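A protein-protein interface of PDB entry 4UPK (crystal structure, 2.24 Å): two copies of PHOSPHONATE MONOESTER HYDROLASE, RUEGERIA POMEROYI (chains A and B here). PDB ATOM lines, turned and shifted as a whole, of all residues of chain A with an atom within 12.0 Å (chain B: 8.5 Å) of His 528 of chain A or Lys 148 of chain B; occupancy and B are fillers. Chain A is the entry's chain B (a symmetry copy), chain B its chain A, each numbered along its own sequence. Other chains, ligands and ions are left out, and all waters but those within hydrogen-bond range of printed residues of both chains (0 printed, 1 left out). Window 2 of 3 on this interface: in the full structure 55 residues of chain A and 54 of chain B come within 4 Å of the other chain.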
ATOM      1  N   CYS A 524      15.178   2.066   2.559  1.00  0.00           N
ATOM      2  CA  CYS A 524      15.077   3.469   2.935  1.00  0.00           C
ATOM      3  C   CYS A 524      14.815   4.245   1.619  1.00  0.00           C
ATOM      4  O   CYS A 524      15.235   3.803   0.534  1.00  0.00           O
ATOM      5  CB  CYS A 524      16.351   3.947   3.634  1.00  0.00           C
ATOM      6  SG  CYS A 524      16.290   5.670   4.214  1.00  0.00           S
ATOM      7  N   SER A 525      14.075   5.361   1.713  1.00  0.00           N
ATOM      8  CA  SER A 525      13.763   6.208   0.565  1.00  0.00           C
ATOM      9  C   SER A 525      13.986   7.684   0.894  1.00  0.00           C
ATOM     10  O   SER A 525      13.510   8.165   1.927  1.00  0.00           O
ATOM     11  CB  SER A 525      12.326   5.985   0.089  1.00  0.00           C
ATOM     12  OG  SER A 525      12.020   4.608  -0.050  1.00  0.00           O
ATOM     13  N   ILE A 526      14.703   8.393  -0.004  1.00  0.00           N
ATOM     14  CA  ILE A 526      14.946   9.836   0.086  1.00  0.00           C
ATOM     15  C   ILE A 526      13.724  10.493  -0.569  1.00  0.00           C
ATOM     16  O   ILE A 526      13.475  10.293  -1.767  1.00  0.00           O
ATOM     17  CB  ILE A 526      16.296  10.272  -0.588  1.00  0.00           C
ATOM     18  CG1 ILE A 526      17.553   9.668   0.106  1.00  0.00           C
ATOM     19  CG2 ILE A 526      16.403  11.806  -0.757  1.00  0.00           C
ATOM     20  CD1 ILE A 526      17.773  10.000   1.684  1.00  0.00           C
ATOM     21  N   THR A 527      12.928  11.215   0.246  1.00  0.00           N
ATOM     22  CA  THR A 527      11.705  11.907  -0.191  1.00  0.00           C
ATOM     23  C   THR A 527      11.891  13.426   0.015  1.00  0.00           C
ATOM     24  O   THR A 527      12.825  13.838   0.725  1.00  0.00           O
ATOM     25  CB  THR A 527      10.447  11.358   0.547  1.00  0.00           C
ATOM     26  OG1 THR A 527      10.326  11.946   1.846  1.00  0.00           O
ATOM     27  CG2 THR A 527      10.424   9.823   0.660  1.00  0.00           C
ATOM     28  N   HIS A 528      10.974  14.242  -0.550  1.00  0.00           N
ATOM     29  CA  HIS A 528      10.976  15.701  -0.426  1.00  0.00           C
ATOM     30  C   HIS A 528      10.887  16.184   1.034  1.00  0.00           C
ATOM     31  O   HIS A 528      11.316  17.305   1.328  1.00  0.00           O
ATOM     32  CB  HIS A 528       9.853  16.308  -1.279  1.00  0.00           C
ATOM     33  CG  HIS A 528       8.477  15.919  -0.834  1.00  0.00           C
ATOM     34  ND1 HIS A 528       7.989  14.637  -1.034  1.00  0.00           N
ATOM     35  CD2 HIS A 528       7.531  16.656  -0.206  1.00  0.00           C
ATOM     36  CE1 HIS A 528       6.771  14.635  -0.518  1.00  0.00           C
ATOM     37  NE2 HIS A 528       6.449  15.828  -0.011  1.00  0.00           N
ATOM     38  N   GLU A 529      10.368  15.318   1.941  1.00  0.00           N
ATOM     39  CA  GLU A 529      10.191  15.565   3.382  1.00  0.00           C
ATOM     40  C   GLU A 529      11.312  14.962   4.252  1.00  0.00           C
ATOM     41  O   GLU A 529      11.345  15.183   5.467  1.00  0.00           O
ATOM     42  CB  GLU A 529       8.829  15.022   3.843  1.00  0.00           C
ATOM     43  CG  GLU A 529       7.636  15.791   3.297  1.00  0.00           C
ATOM     44  CD  GLU A 529       6.296  15.079   3.344  1.00  0.00           C
ATOM     45  OE1 GLU A 529       6.116  14.169   4.188  1.00  0.00           O
ATOM     46  OE2 GLU A 529       5.413  15.451   2.539  1.00  0.00           O
ATOM     47  N   GLY A 530      12.210  14.216   3.625  1.00  0.00           N
ATOM     48  CA  GLY A 530      13.318  13.557   4.306  1.00  0.00           C
ATOM     49  C   GLY A 530      13.373  12.073   4.009  1.00  0.00           C
ATOM     50  O   GLY A 530      12.666  11.582   3.119  1.00  0.00           O
ATOM     51  N   ALA A 531      14.229  11.344   4.755  1.00  0.00           N
ATOM     52  CA  ALA A 531      14.403   9.899   4.578  1.00  0.00           C
ATOM     53  C   ALA A 531      13.299   9.123   5.306  1.00  0.00           C
ATOM     54  O   ALA A 531      12.987   9.413   6.462  1.00  0.00           O
ATOM     55  CB  ALA A 531      15.781   9.458   5.053  1.00  0.00           C
ATOM     56  N   ARG A 532      12.675   8.177   4.598  1.00  0.00           N
ATOM     57  CA  ARG A 532      11.604   7.357   5.145  1.00  0.00           C
ATOM     58  C   ARG A 532      11.962   5.891   4.944  1.00  0.00           C
ATOM     59  O   ARG A 532      12.451   5.523   3.879  1.00  0.00           O
ATOM     60  CB  ARG A 532      10.243   7.694   4.504  1.00  0.00           C
ATOM     61  CG  ARG A 532       9.741   9.138   4.693  1.00  0.00           C
ATOM     62  CD  ARG A 532       9.313   9.437   6.120  1.00  0.00           C
ATOM     63  NE  ARG A 532       8.674  10.752   6.239  1.00  0.00           N
ATOM     64  CZ  ARG A 532       9.285  11.875   6.610  1.00  0.00           C
ATOM     65  NH1 ARG A 532      10.593  11.884   6.849  1.00  0.00           N
ATOM     66  NH2 ARG A 532       8.604  13.006   6.703  1.00  0.00           N
ATOM     67  N   THR A 533      11.735   5.058   5.972  1.00  0.00           N
ATOM     68  CA  THR A 533      12.063   3.634   5.920  1.00  0.00           C
ATOM     69  C   THR A 533      10.851   2.710   5.859  1.00  0.00           C
ATOM     70  O   THR A 533       9.786   3.045   6.375  1.00  0.00           O
ATOM     71  CB  THR A 533      13.096   3.249   7.002  1.00  0.00           C
ATOM     72  OG1 THR A 533      13.669   1.976   6.675  1.00  0.00           O
ATOM     73  CG2 THR A 533      12.502   3.233   8.421  1.00  0.00           C
ATOM     74  N   THR B 133      22.907  11.729  -6.407  1.00  0.00           N
ATOM     75  CA  THR B 133      23.275  10.862  -5.295  1.00  0.00           C
ATOM     76  C   THR B 133      22.310  10.977  -4.109  1.00  0.00           C
ATOM     77  O   THR B 133      22.101  12.070  -3.569  1.00  0.00           O
ATOM     78  CB  THR B 133      24.744  11.046  -4.887  1.00  0.00           C
ATOM     79  OG1 THR B 133      25.557  11.211  -6.044  1.00  0.00           O
ATOM     80  CG2 THR B 133      25.274   9.876  -4.046  1.00  0.00           C
ATOM     81  N   SER B 134      21.749   9.822  -3.702  1.00  0.00           N
ATOM     82  CA  SER B 134      20.878   9.717  -2.545  1.00  0.00           C
ATOM     83  C   SER B 134      21.811   9.544  -1.353  1.00  0.00           C
ATOM     84  O   SER B 134      22.589   8.583  -1.290  1.00  0.00           O
ATOM     85  CB  SER B 134      19.942   8.529  -2.698  1.00  0.00           C
ATOM     86  OG  SER B 134      19.220   8.623  -3.911  1.00  0.00           O
ATOM     87  N   GLN B 135      21.799  10.528  -0.460  1.00  0.00           N
ATOM     88  CA  GLN B 135      22.694  10.554   0.693  1.00  0.00           C
ATOM     89  C   GLN B 135      22.328   9.558   1.790  1.00  0.00           C
ATOM     90  O   GLN B 135      21.171   9.139   1.895  1.00  0.00           O
ATOM     91  CB  GLN B 135      22.880  11.993   1.237  1.00  0.00           C
ATOM     92  CG  GLN B 135      23.191  13.056   0.170  1.00  0.00           C
ATOM     93  CD  GLN B 135      24.434  12.814  -0.661  1.00  0.00           C
ATOM     94  OE1 GLN B 135      25.540  12.652  -0.145  1.00  0.00           O
ATOM     95  NE2 GLN B 135      24.294  12.868  -1.978  1.00  0.00           N
ATOM     96  N   TYR B 140      23.930  12.344   8.170  1.00  0.00           N
ATOM     97  CA  TYR B 140      23.342  13.684   8.278  1.00  0.00           C
ATOM     98  C   TYR B 140      22.252  13.814   9.343  1.00  0.00           C
ATOM     99  O   TYR B 140      21.628  12.819   9.714  1.00  0.00           O
ATOM    100  CB  TYR B 140      22.728  14.086   6.926  1.00  0.00           C
ATOM    101  CG  TYR B 140      23.712  14.325   5.809  1.00  0.00           C
ATOM    102  CD1 TYR B 140      24.116  13.284   4.975  1.00  0.00           C
ATOM    103  CD2 TYR B 140      24.146  15.611   5.504  1.00  0.00           C
ATOM    104  CE1 TYR B 140      24.986  13.507   3.909  1.00  0.00           C
ATOM    105  CE2 TYR B 140      25.007  15.848   4.433  1.00  0.00           C
ATOM    106  CZ  TYR B 140      25.421  14.793   3.635  1.00  0.00           C
ATOM    107  OH  TYR B 140      26.270  15.021   2.581  1.00  0.00           O
ATOM    108  N   ASP B 141      21.961  15.076   9.768  1.00  0.00           N
ATOM    109  CA  ASP B 141      20.846  15.398  10.671  1.00  0.00           C
ATOM    110  C   ASP B 141      19.557  15.083   9.884  1.00  0.00           C
ATOM    111  O   ASP B 141      19.532  15.303   8.670  1.00  0.00           O
ATOM    112  CB  ASP B 141      20.872  16.890  11.089  1.00  0.00           C
ATOM    113  CG  ASP B 141      19.621  17.361  11.816  1.00  0.00           C
ATOM    114  OD1 ASP B 141      19.314  16.808  12.900  1.00  0.00           O
ATOM    115  OD2 ASP B 141      18.947  18.272  11.302  1.00  0.00           O
ATOM    116  N   ALA B 142      18.509  14.552  10.567  1.00  0.00           N
ATOM    117  CA  ALA B 142      17.208  14.193   9.965  1.00  0.00           C
ATOM    118  C   ALA B 142      16.601  15.289   9.076  1.00  0.00           C
ATOM    119  O   ALA B 142      16.064  14.965   8.015  1.00  0.00           O
ATOM    120  CB  ALA B 142      16.218  13.795  11.056  1.00  0.00           C
ATOM    121  N   ASN B 143      16.734  16.578   9.494  1.00  0.00           N
ATOM    122  CA  ASN B 143      16.220  17.761   8.789  1.00  0.00           C
ATOM    123  C   ASN B 143      17.196  18.426   7.759  1.00  0.00           C
ATOM    124  O   ASN B 143      16.887  19.482   7.207  1.00  0.00           O
ATOM    125  CB  ASN B 143      15.664  18.790   9.800  1.00  0.00           C
ATOM    126  CG  ASN B 143      14.752  19.832   9.178  1.00  0.00           C
ATOM    127  OD1 ASN B 143      13.981  19.544   8.246  1.00  0.00           O
ATOM    128  ND2 ASN B 143      14.842  21.075   9.652  1.00  0.00           N
ATOM    129  N   ASP B 144      18.341  17.796   7.485  1.00  0.00           N
ATOM    130  CA  ASP B 144      19.327  18.303   6.523  1.00  0.00           C
ATOM    131  C   ASP B 144      18.774  18.400   5.077  1.00  0.00           C
ATOM    132  O   ASP B 144      18.141  17.443   4.609  1.00  0.00           O
ATOM    133  CB  ASP B 144      20.580  17.406   6.532  1.00  0.00           C
ATOM    134  CG  ASP B 144      21.843  18.121   6.114  1.00  0.00           C
ATOM    135  OD1 ASP B 144      22.014  18.355   4.898  1.00  0.00           O
ATOM    136  OD2 ASP B 144      22.669  18.444   7.007  1.00  0.00           O
ATOM    137  N   PRO B 145      19.060  19.519   4.340  1.00  0.00           N
ATOM    138  CA  PRO B 145      18.605  19.617   2.935  1.00  0.00           C
ATOM    139  C   PRO B 145      19.062  18.444   2.054  1.00  0.00           C
ATOM    140  O   PRO B 145      18.300  18.005   1.199  1.00  0.00           O
ATOM    141  CB  PRO B 145      19.220  20.940   2.450  1.00  0.00           C
ATOM    142  CG  PRO B 145      19.480  21.727   3.696  1.00  0.00           C
ATOM    143  CD  PRO B 145      19.798  20.739   4.758  1.00  0.00           C
ATOM    144  N   ALA B 146      20.283  17.921   2.294  1.00  0.00           N
ATOM    145  CA  ALA B 146      20.916  16.786   1.601  1.00  0.00           C
ATOM    146  C   ALA B 146      20.074  15.505   1.603  1.00  0.00           C
ATOM    147  O   ALA B 146      20.265  14.647   0.730  1.00  0.00           O
ATOM    148  CB  ALA B 146      22.273  16.497   2.201  1.00  0.00           C
ATOM    149  N   LEU B 147      19.156  15.371   2.595  1.00  0.00           N
ATOM    150  CA  LEU B 147      18.260  14.222   2.727  1.00  0.00           C
ATOM    151  C   LEU B 147      16.854  14.496   2.141  1.00  0.00           C
ATOM    152  O   LEU B 147      15.952  13.686   2.321  1.00  0.00           O
ATOM    153  CB  LEU B 147      18.180  13.756   4.211  1.00  0.00           C
ATOM    154  CG  LEU B 147      19.480  13.272   4.886  1.00  0.00           C
ATOM    155  CD1 LEU B 147      19.208  12.889   6.313  1.00  0.00           C
ATOM    156  CD2 LEU B 147      20.103  12.077   4.131  1.00  0.00           C
ATOM    157  N   LYS B 148      16.669  15.637   1.467  1.00  0.00           N
ATOM    158  CA  LYS B 148      15.371  16.015   0.883  1.00  0.00           C
ATOM    159  C   LYS B 148      15.328  15.881  -0.639  1.00  0.00           C
ATOM    160  O   LYS B 148      14.270  16.010  -1.244  1.00  0.00           O
ATOM    161  CB  LYS B 148      14.940  17.413   1.349  1.00  0.00           C
ATOM    162  CG  LYS B 148      14.493  17.432   2.788  1.00  0.00           C
ATOM    163  CD  LYS B 148      13.835  18.758   3.147  1.00  0.00           C
ATOM    164  CE  LYS B 148      13.534  18.830   4.626  1.00  0.00           C
ATOM    165  NZ  LYS B 148      14.776  18.909   5.448  1.00  0.00           N
ATOM    166  N   THR B 149      16.475  15.571  -1.248  1.00  0.00           N
ATOM    167  CA  THR B 149      16.595  15.403  -2.697  1.00  0.00           C
ATOM    168  C   THR B 149      17.543  14.264  -3.079  1.00  0.00           C
ATOM    169  O   THR B 149      18.589  14.112  -2.448  1.00  0.00           O
ATOM    170  CB  THR B 149      16.966  16.748  -3.375  1.00  0.00           C
ATOM    171  OG1 THR B 149      16.997  16.560  -4.788  1.00  0.00           O
ATOM    172  CG2 THR B 149      18.303  17.333  -2.880  1.00  0.00           C
ATOM    173  N   TYR B 150      17.177  13.474  -4.117  1.00  0.00           N
ATOM    174  CA  TYR B 150      18.044  12.415  -4.610  1.00  0.00           C
ATOM    175  C   TYR B 150      18.917  12.882  -5.785  1.00  0.00           C
ATOM    176  O   TYR B 150      19.527  12.066  -6.475  1.00  0.00           O
ATOM    177  CB  TYR B 150      17.292  11.101  -4.880  1.00  0.00           C
ATOM    178  CG  TYR B 150      16.190  11.131  -5.922  1.00  0.00           C
ATOM    179  CD1 TYR B 150      16.488  11.241  -7.280  1.00  0.00           C
ATOM    180  CD2 TYR B 150      14.867  10.871  -5.570  1.00  0.00           C
ATOM    181  CE1 TYR B 150      15.486  11.214  -8.249  1.00  0.00           C
ATOM    182  CE2 TYR B 150      13.857  10.817  -6.534  1.00  0.00           C
ATOM    183  CZ  TYR B 150      14.172  10.998  -7.873  1.00  0.00           C
ATOM    184  OH  TYR B 150      13.193  10.948  -8.839  1.00  0.00           O
ATOM    185  N   GLU B 151      18.979  14.207  -5.990  1.00  0.00           N
ATOM    186  CA  GLU B 151      19.762  14.886  -7.019  1.00  0.00           C
ATOM    187  C   GLU B 151      21.002  15.535  -6.397  1.00  0.00           C
ATOM    188  O   GLU B 151      21.788  16.179  -7.107  1.00  0.00           O
ATOM    189  CB  GLU B 151      18.924  15.996  -7.656  1.00  0.00           C
ATOM    190  CG  GLU B 151      17.704  15.580  -8.449  1.00  0.00           C
ATOM    191  CD  GLU B 151      17.098  16.786  -9.138  1.00  0.00           C
ATOM    192  OE1 GLU B 151      16.747  17.772  -8.446  1.00  0.00           O
ATOM    193  OE2 GLU B 151      17.047  16.772 -10.387  1.00  0.00           O
ATOM    194  N   PHE B 152      21.150  15.391  -5.066  1.00  0.00           N
ATOM    195  CA  PHE B 152      22.222  15.968  -4.258  1.00  0.00           C
ATOM    196  C   PHE B 152      23.658  15.540  -4.681  1.00  0.00           C
ATOM    197  O   PHE B 152      23.849  14.360  -5.001  1.00  0.00           O
ATOM    198  CB  PHE B 152      21.967  15.704  -2.762  1.00  0.00           C
ATOM    199  CG  PHE B 152      22.597  16.750  -1.875  1.00  0.00           C
ATOM    200  CD1 PHE B 152      22.006  17.999  -1.718  1.00  0.00           C
ATOM    201  CD2 PHE B 152      23.822  16.513  -1.254  1.00  0.00           C
ATOM    202  CE1 PHE B 152      22.617  18.988  -0.942  1.00  0.00           C
ATOM    203  CE2 PHE B 152      24.444  17.506  -0.496  1.00  0.00           C
ATOM    204  CZ  PHE B 152      23.833  18.736  -0.331  1.00  0.00           C
ATOM    205  N   ARG B 164      20.943  20.540 -11.590  1.00  0.00           N
ATOM    206  CA  ARG B 164      20.115  19.357 -11.460  1.00  0.00           C
ATOM    207  C   ARG B 164      18.759  19.733 -12.069  1.00  0.00           C
ATOM    208  O   ARG B 164      18.272  20.839 -11.830  1.00  0.00           O
ATOM    209  CB  ARG B 164      19.944  18.968  -9.978  1.00  0.00           C
ATOM    210  CG  ARG B 164      21.221  19.008  -9.175  1.00  0.00           C
ATOM    211  CD  ARG B 164      20.909  19.188  -7.707  1.00  0.00           C
ATOM    212  NE  ARG B 164      21.971  19.939  -7.044  1.00  0.00           N
ATOM    213  CZ  ARG B 164      22.042  20.138  -5.736  1.00  0.00           C
ATOM    214  NH1 ARG B 164      21.118  19.631  -4.929  1.00  0.00           N
ATOM    215  NH2 ARG B 164      23.035  20.847  -5.222  1.00  0.00           N
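O of Thr 527 of chain A lies close to O of Lys 148 of chain B.
O of Thr 133 of chain B lies within hydrogen-bond range of NE2 of Gln 135 of chain B, 2.8 Å away. The backbone NH (N) of Glu 529 of chain A lies close to the side-chain hydroxyl (OG1) of Thr 527 of chain A. The side-chain hydroxyl (OG1) of Thr 149 of chain B sits close to the backbone NH (N) of Glu 151 of chain B. A ring nitrogen (NE2) of His 528 of chain A lies within hydrogen-bond range of the side-chain carboxylate (OE2) of Glu 529 of chain A, 2.8 Å away. OG1 of Thr 527 of chain A sits at hydrogen-bond distance from O of Gly 530 of chain A. The backbone carbonyl oxygen (O) of Phe 152 of chain B lies within hydrogen-bond range of the side-chain amide nitrogen (NE2) of Gln 135 of chain B, at 3.4 Å.
CB of Ser 134 of chain B touches CG1 of Ile 526 of chain A, 3.9 Å away. O of Gln 135 of chain B touches CD1 of Ile 526 of chain A, 3.5 Å away. Leu 147 of chain B touches Ile 526 of chain A (O to CG2, 3.6 Å). Thr 149 of chain B touches Ile 526 of chain A. CG2 of Ile 526 of chain A touches N of Tyr 150 of chain B (3.8 Å). Leu 147 of chain B touches Thr 527 of chain A. Lys 148 of chain B touches His 528 of chain A (O to CA, 3.4 Å). Leu 147 of chain B touches Gly 530 of chain A. Ala 531 of chain A touches Leu 147 of chain B (N to O, 3.8 Å).
His 528 of chain A touches just one residue of chain B: Lys 148 (3.4 Å). Lys 148 of chain B touches just these residues of chain A: Thr 527 and His 528. No residue of chain A comes within 4 Å of Ala 142 of chain B. No residue of chain A comes within 4 Å of Asn 143 of chain B. No residue of chain A comes within 4 Å of Pro 145 of chain B. No residue of chain A comes within 4 Å of Ala 146 of chain B. Of chain A, only Ile 526 (3.6 Å), Thr 527 (3.5 Å), Gly 530 (3.3 Å) and Ala 531 (3.8 Å) come within 4 Å of Leu 147 of chain B. Printed residues of chain B within 4 Å of Ile 526 of chain A: Ser 134 (3.9 Å), Gln 135 (3.5 Å), Leu 147 (3.6 Å), Thr 149 (3.6 Å) and Tyr 150 (3.8 Å). Of the printed residues of chain A, Tyr 150 of chain B touches Ile 526 (3.8 Å). Of the printed residues of chain B, Thr 527 of chain A touches Leu 147 (3.5 Å) and Lys 148 (3.3 Å). The nearest printed residue of chain B that does not touch Thr 527 of chain A is Thr 149 of chain B (4.5 Å).
Printed residues of chain A that touch a printed residue of chain B: Ile 526, Thr 527, His 528, Gly 530 and Ala 531. Hydrophobic or aromatic side chains of chain A that line the printed part of chain B: Ile 526. Of the 17 printed residues of chain B, 6 touch a printed residue of chain A. Hydrophobic or aromatic side chains of chain B within 4 Å of the printed part of chain A: Leu 147. Along chain B the printed residues that touch a printed residue of chain A span positions 134 to 150. Among the printed residues, no Asp or Glu carboxylate lies within 4 Å of a Lys or Arg side-chain nitrogen of the other chain.
No position is printed for both chains. Of the 10 pairs that touch across the chains among the printed residues, none has its exchanged pair printed and touching as well.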
